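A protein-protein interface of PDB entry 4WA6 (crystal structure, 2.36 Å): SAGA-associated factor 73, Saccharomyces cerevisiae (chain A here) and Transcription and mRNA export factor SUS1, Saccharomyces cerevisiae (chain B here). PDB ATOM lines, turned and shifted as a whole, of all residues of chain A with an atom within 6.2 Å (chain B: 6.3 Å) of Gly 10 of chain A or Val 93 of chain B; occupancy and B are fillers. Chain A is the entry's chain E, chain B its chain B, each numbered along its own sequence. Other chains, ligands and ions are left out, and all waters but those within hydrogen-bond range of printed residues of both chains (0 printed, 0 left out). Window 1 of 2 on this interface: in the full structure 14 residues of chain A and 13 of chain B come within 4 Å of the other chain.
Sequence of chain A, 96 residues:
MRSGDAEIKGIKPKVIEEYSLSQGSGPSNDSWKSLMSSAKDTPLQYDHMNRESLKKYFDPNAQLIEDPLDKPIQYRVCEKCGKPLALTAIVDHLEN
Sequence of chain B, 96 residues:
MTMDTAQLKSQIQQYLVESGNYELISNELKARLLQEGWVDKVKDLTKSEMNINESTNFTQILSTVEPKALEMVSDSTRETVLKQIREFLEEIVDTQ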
ATOM      1  N   ILE A   8     -27.965  26.987 -18.180  1.00  0.00           N
ATOM      2  CA  ILE A   8     -27.739  25.724 -18.836  1.00  0.00           C
ATOM      3  C   ILE A   8     -28.412  24.542 -18.095  1.00  0.00           C
ATOM      4  O   ILE A   8     -28.041  24.182 -16.982  1.00  0.00           O
ATOM      5  CB  ILE A   8     -26.236  25.489 -18.991  1.00  0.00           C
ATOM      6  CG1 ILE A   8     -25.678  26.518 -19.969  1.00  0.00           C
ATOM      7  CG2 ILE A   8     -25.966  24.073 -19.465  1.00  0.00           C
ATOM      8  CD1 ILE A   8     -24.219  26.339 -20.337  1.00  0.00           C
ATOM      9  N   LYS A   9     -29.403  23.948 -18.742  1.00  0.00           N
ATOM     10  CA  LYS A   9     -30.067  22.737 -18.249  1.00  0.00           C
ATOM     11  C   LYS A   9     -29.156  21.498 -18.106  1.00  0.00           C
ATOM     12  O   LYS A   9     -29.134  20.834 -17.081  1.00  0.00           O
ATOM     13  CB  LYS A   9     -31.217  22.386 -19.208  1.00  0.00           C
ATOM     14  CG  LYS A   9     -32.518  22.025 -18.522  1.00  0.00           C
ATOM     15  CD  LYS A   9     -33.608  21.773 -19.556  1.00  0.00           C
ATOM     16  CE  LYS A   9     -34.925  22.417 -19.156  1.00  0.00           C
ATOM     17  NZ  LYS A   9     -35.814  22.551 -20.337  1.00  0.00           N
ATOM     18  N   GLY A  10     -28.416  21.189 -19.166  1.00  0.00           N
ATOM     19  CA  GLY A  10     -27.687  19.919 -19.295  1.00  0.00           C
ATOM     20  C   GLY A  10     -27.128  19.804 -20.697  1.00  0.00           C
ATOM     21  O   GLY A  10     -27.293  20.685 -21.504  1.00  0.00           O
ATOM     22  N   ILE A  11     -26.481  18.694 -20.982  1.00  0.00           N
ATOM     23  CA  ILE A  11     -25.928  18.406 -22.303  1.00  0.00           C
ATOM     24  C   ILE A  11     -26.991  17.813 -23.201  1.00  0.00           C
ATOM     25  O   ILE A  11     -27.787  17.029 -22.761  1.00  0.00           O
ATOM     26  CB  ILE A  11     -24.718  17.464 -22.167  1.00  0.00           C
ATOM     27  CG1 ILE A  11     -23.549  18.309 -21.721  1.00  0.00           C
ATOM     28  CG2 ILE A  11     -24.349  16.845 -23.489  1.00  0.00           C
ATOM     29  CD1 ILE A  11     -22.427  17.526 -21.131  1.00  0.00           C
ATOM     30  N   LYS A  12     -27.028  18.201 -24.464  1.00  0.00           N
ATOM     31  CA  LYS A  12     -28.104  17.726 -25.323  1.00  0.00           C
ATOM     32  C   LYS A  12     -28.011  16.222 -25.421  1.00  0.00           C
ATOM     33  O   LYS A  12     -26.899  15.694 -25.661  1.00  0.00           O
ATOM     34  CB  LYS A  12     -27.980  18.270 -26.735  1.00  0.00           C
ATOM     35  CG  LYS A  12     -28.121  19.765 -26.923  1.00  0.00           C
ATOM     36  CD  LYS A  12     -28.250  20.038 -28.427  1.00  0.00           C
ATOM     37  CE  LYS A  12     -28.144  21.511 -28.757  1.00  0.00           C
ATOM     38  NZ  LYS A  12     -28.962  22.317 -27.804  1.00  0.00           N
ATOM     39  N   VAL A  15     -26.454  14.954 -28.486  1.00  0.00           N
ATOM     40  CA  VAL A  15     -24.987  14.915 -28.498  1.00  0.00           C
ATOM     41  C   VAL A  15     -24.416  13.752 -27.678  1.00  0.00           C
ATOM     42  O   VAL A  15     -23.335  13.243 -27.985  1.00  0.00           O
ATOM     43  CB  VAL A  15     -24.355  16.239 -27.942  1.00  0.00           C
ATOM     44  CG1 VAL A  15     -22.835  16.148 -27.882  1.00  0.00           C
ATOM     45  CG2 VAL A  15     -24.757  17.454 -28.774  1.00  0.00           C
ATOM     46  N   LEU B   8     -21.130  19.171 -14.513  1.00  0.00           N
ATOM     47  CA  LEU B   8     -21.611  19.614 -15.772  1.00  0.00           C
ATOM     48  C   LEU B   8     -20.582  20.509 -16.472  1.00  0.00           C
ATOM     49  O   LEU B   8     -20.363  20.380 -17.662  1.00  0.00           O
ATOM     50  CB  LEU B   8     -22.955  20.335 -15.616  1.00  0.00           C
ATOM     51  CG  LEU B   8     -23.757  20.612 -16.885  1.00  0.00           C
ATOM     52  CD1 LEU B   8     -23.594  19.463 -17.869  1.00  0.00           C
ATOM     53  CD2 LEU B   8     -25.239  20.841 -16.569  1.00  0.00           C
ATOM     54  N   ILE B  12     -18.910  19.680 -20.246  1.00  0.00           N
ATOM     55  CA  ILE B  12     -18.949  20.584 -21.368  1.00  0.00           C
ATOM     56  C   ILE B  12     -17.533  20.739 -21.973  1.00  0.00           C
ATOM     57  O   ILE B  12     -17.308  20.536 -23.185  1.00  0.00           O
ATOM     58  CB  ILE B  12     -19.597  21.915 -20.961  1.00  0.00           C
ATOM     59  CG1 ILE B  12     -21.084  21.722 -20.662  1.00  0.00           C
ATOM     60  CG2 ILE B  12     -19.489  22.930 -22.069  1.00  0.00           C
ATOM     61  CD1 ILE B  12     -21.779  22.986 -20.180  1.00  0.00           C
ATOM     62  N   PHE B  88     -19.939  27.132 -30.300  1.00  0.00           N
ATOM     63  CA  PHE B  88     -19.688  25.737 -30.028  1.00  0.00           C
ATOM     64  C   PHE B  88     -20.487  25.222 -28.829  1.00  0.00           C
ATOM     65  O   PHE B  88     -20.996  24.100 -28.856  1.00  0.00           O
ATOM     66  CB  PHE B  88     -18.189  25.489 -29.792  1.00  0.00           C
ATOM     67  CG  PHE B  88     -17.327  25.590 -31.039  1.00  0.00           C
ATOM     68  CD1 PHE B  88     -17.676  24.939 -32.207  1.00  0.00           C
ATOM     69  CD2 PHE B  88     -16.127  26.270 -31.011  1.00  0.00           C
ATOM     70  CE1 PHE B  88     -16.872  25.014 -33.339  1.00  0.00           C
ATOM     71  CE2 PHE B  88     -15.307  26.334 -32.125  1.00  0.00           C
ATOM     72  CZ  PHE B  88     -15.688  25.717 -33.299  1.00  0.00           C
ATOM     73  N   LEU B  89     -20.605  26.019 -27.775  1.00  0.00           N
ATOM     74  CA  LEU B  89     -21.460  25.662 -26.660  1.00  0.00           C
ATOM     75  C   LEU B  89     -22.902  25.492 -27.052  1.00  0.00           C
ATOM     76  O   LEU B  89     -23.559  24.653 -26.483  1.00  0.00           O
ATOM     77  CB  LEU B  89     -21.398  26.690 -25.529  1.00  0.00           C
ATOM     78  CG  LEU B  89     -20.110  26.783 -24.715  1.00  0.00           C
ATOM     79  CD1 LEU B  89     -20.244  27.838 -23.623  1.00  0.00           C
ATOM     80  CD2 LEU B  89     -19.782  25.431 -24.129  1.00  0.00           C
ATOM     81  N   GLU B  90     -23.414  26.265 -27.997  1.00  0.00           N
ATOM     82  CA  GLU B  90     -24.830  26.105 -28.419  1.00  0.00           C
ATOM     83  C   GLU B  90     -25.065  24.791 -29.171  1.00  0.00           C
ATOM     84  O   GLU B  90     -26.161  24.291 -29.172  1.00  0.00           O
ATOM     85  CB  GLU B  90     -25.354  27.333 -29.202  1.00  0.00           C
ATOM     86  CG  GLU B  90     -25.785  28.466 -28.262  1.00  0.00           C
ATOM     87  CD  GLU B  90     -25.656  29.891 -28.823  1.00  0.00           C
ATOM     88  OE1 GLU B  90     -25.099  30.068 -29.934  1.00  0.00           O
ATOM     89  OE2 GLU B  90     -26.103  30.853 -28.135  1.00  0.00           O
ATOM     90  N   GLU B  91     -24.018  24.208 -29.748  1.00  0.00           N
ATOM     91  CA  GLU B  91     -24.115  22.855 -30.335  1.00  0.00           C
ATOM     92  C   GLU B  91     -24.236  21.749 -29.284  1.00  0.00           C
ATOM     93  O   GLU B  91     -24.749  20.692 -29.582  1.00  0.00           O
ATOM     94  CB  GLU B  91     -22.882  22.529 -31.207  1.00  0.00           C
ATOM     95  CG  GLU B  91     -22.619  23.497 -32.348  1.00  0.00           C
ATOM     96  CD  GLU B  91     -21.335  23.202 -33.158  1.00  0.00           C
ATOM     97  OE1 GLU B  91     -20.548  22.236 -32.877  1.00  0.00           O
ATOM     98  OE2 GLU B  91     -21.114  23.971 -34.127  1.00  0.00           O
ATOM     99  N   ILE B  92     -23.714  21.984 -28.083  1.00  0.00           N
ATOM    100  CA  ILE B  92     -23.510  20.964 -27.074  1.00  0.00           C
ATOM    101  C   ILE B  92     -24.623  20.941 -26.007  1.00  0.00           C
ATOM    102  O   ILE B  92     -24.976  19.872 -25.523  1.00  0.00           O
ATOM    103  CB  ILE B  92     -22.134  21.207 -26.396  1.00  0.00           C
ATOM    104  CG1 ILE B  92     -20.984  20.875 -27.360  1.00  0.00           C
ATOM    105  CG2 ILE B  92     -21.953  20.387 -25.121  1.00  0.00           C
ATOM    106  CD1 ILE B  92     -19.662  21.464 -26.927  1.00  0.00           C
ATOM    107  N   VAL B  93     -25.180  22.101 -25.631  1.00  0.00           N
ATOM    108  CA  VAL B  93     -25.975  22.201 -24.374  1.00  0.00           C
ATOM    109  C   VAL B  93     -27.418  22.607 -24.553  1.00  0.00           C
ATOM    110  O   VAL B  93     -27.772  23.100 -25.596  1.00  0.00           O
ATOM    111  CB  VAL B  93     -25.356  23.183 -23.339  1.00  0.00           C
ATOM    112  CG1 VAL B  93     -23.941  22.767 -23.010  1.00  0.00           C
ATOM    113  CG2 VAL B  93     -25.400  24.626 -23.824  1.00  0.00           C
ATOM    114  N   ASP B  94     -28.231  22.392 -23.513  1.00  0.00           N
ATOM    115  CA  ASP B  94     -29.618  22.853 -23.465  1.00  0.00           C
ATOM    116  C   ASP B  94     -29.830  23.860 -22.361  1.00  0.00           C
ATOM    117  O   ASP B  94     -29.365  23.653 -21.256  1.00  0.00           O
ATOM    118  CB  ASP B  94     -30.549  21.676 -23.188  1.00  0.00           C
ATOM    119  CG  ASP B  94     -31.012  21.013 -24.435  1.00  0.00           C
ATOM    120  OD1 ASP B  94     -31.466  21.739 -25.348  1.00  0.00           O
ATOM    121  OD2 ASP B  94     -30.913  19.778 -24.499  1.00  0.00           O
ATOM    122  N   THR B  95     -30.600  24.900 -22.647  1.00  0.00           N
ATOM    123  CA  THR B  95     -30.715  26.040 -21.765  1.00  0.00           C
ATOM    124  C   THR B  95     -32.156  26.334 -21.426  1.00  0.00           C
ATOM    125  O   THR B  95     -33.072  25.889 -22.102  1.00  0.00           O
ATOM    126  CB  THR B  95     -30.142  27.284 -22.427  1.00  0.00           C
ATOM    127  OG1 THR B  95     -30.841  27.509 -23.641  1.00  0.00           O
ATOM    128  CG2 THR B  95     -28.689  27.097 -22.776  1.00  0.00           C
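Printed residues of chain B within 4 Å of Ile 8 of chain A: Asp 94.
Gly 10 of chain A touches three residues of chain B.
Of the printed residues of chain B, Ile 11 of chain A touches Leu 8 and Ile 92.
Of the printed residues of chain B, Val 15 of chain A touches Glu 91 (3.3 Å).
Val 93 of chain B touches just these residues of chain A: Gly 10 (3.5 Å) and Lys 12 (2.6 Å).
Printed residues of chain A within 4 Å of Thr 95 of chain B: Lys 9.
The nearest residue of chain B that does not touch Gly 10 of chain A is Ile 92 of chain B (4.7 Å).
The nearest residue of chain A that does not touch Val 93 of chain B is Ile 8 of chain A (4.02 Å).
C of Ile 8 of chain A touches O of Asp 94 of chain B, at 3.4 Å.
CD2 of Leu 8 of chain B touches O of Lys 9 of chain A, 3.9 Å away.
Lys 9 of chain A touches Thr 95 of chain B.
Gly 10 of chain A touches Leu 8 of chain B.
O of Gly 10 of chain A touches CA of Val 93 of chain B, 3.5 Å away.
Ile 11 of chain A touches Leu 8 of chain B (CD1 to CD1, 3.97 Å).
Ile 11 of chain A touches Ile 92 of chain B.
Lys 12 of chain A touches Glu 90 of chain B.
Glu 91 of chain B touches Lys 12 of chain A.
Val 15 of chain A touches Glu 91 of chain B.
N of Asp 94 of chain B lies within hydrogen-bond range of O of Gly 10 of chain A (2.8 Å).
OD1 of Asp 94 of chain B lies within salt-bridge range of NZ of Lys 12 of chain A (3.6 Å).
The backbone NH (N) of Lys 12 of chain A sits at hydrogen-bond distance from the backbone carbonyl oxygen (O) of Ile 92 of chain B.
The backbone NH (N) of Lys 9 of chain A sits at hydrogen-bond distance from the backbone carbonyl oxygen (O) of Asp 94 of chain B, at 2.5 Å.
The backbone carbonyl oxygen of Val 93 of chain B lies within hydrogen-bond range of the side-chain amino group of Lys 12 of chain A, 2.6 Å away.
Printed residues of chain A that touch a printed residue of chain B: Ile 8, Lys 9, Gly 10, Ile 11, Lys 12 and Val 15.
Hydrophobic or aromatic side chains of chain A within 4 Å of the printed part of chain B: Ile 8, Ile 11 and Val 15.
Printed residues of chain B that touch a printed residue of chain A: Leu 8, Glu 90, Glu 91, Ile 92, Val 93, Asp 94 and Thr 95.
Among the printed residues, Asp or Glu carboxylates within 4 Å of a Lys or Arg side-chain nitrogen of the other chain: Lys 12 of chain A with Asp 94 of chain B.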
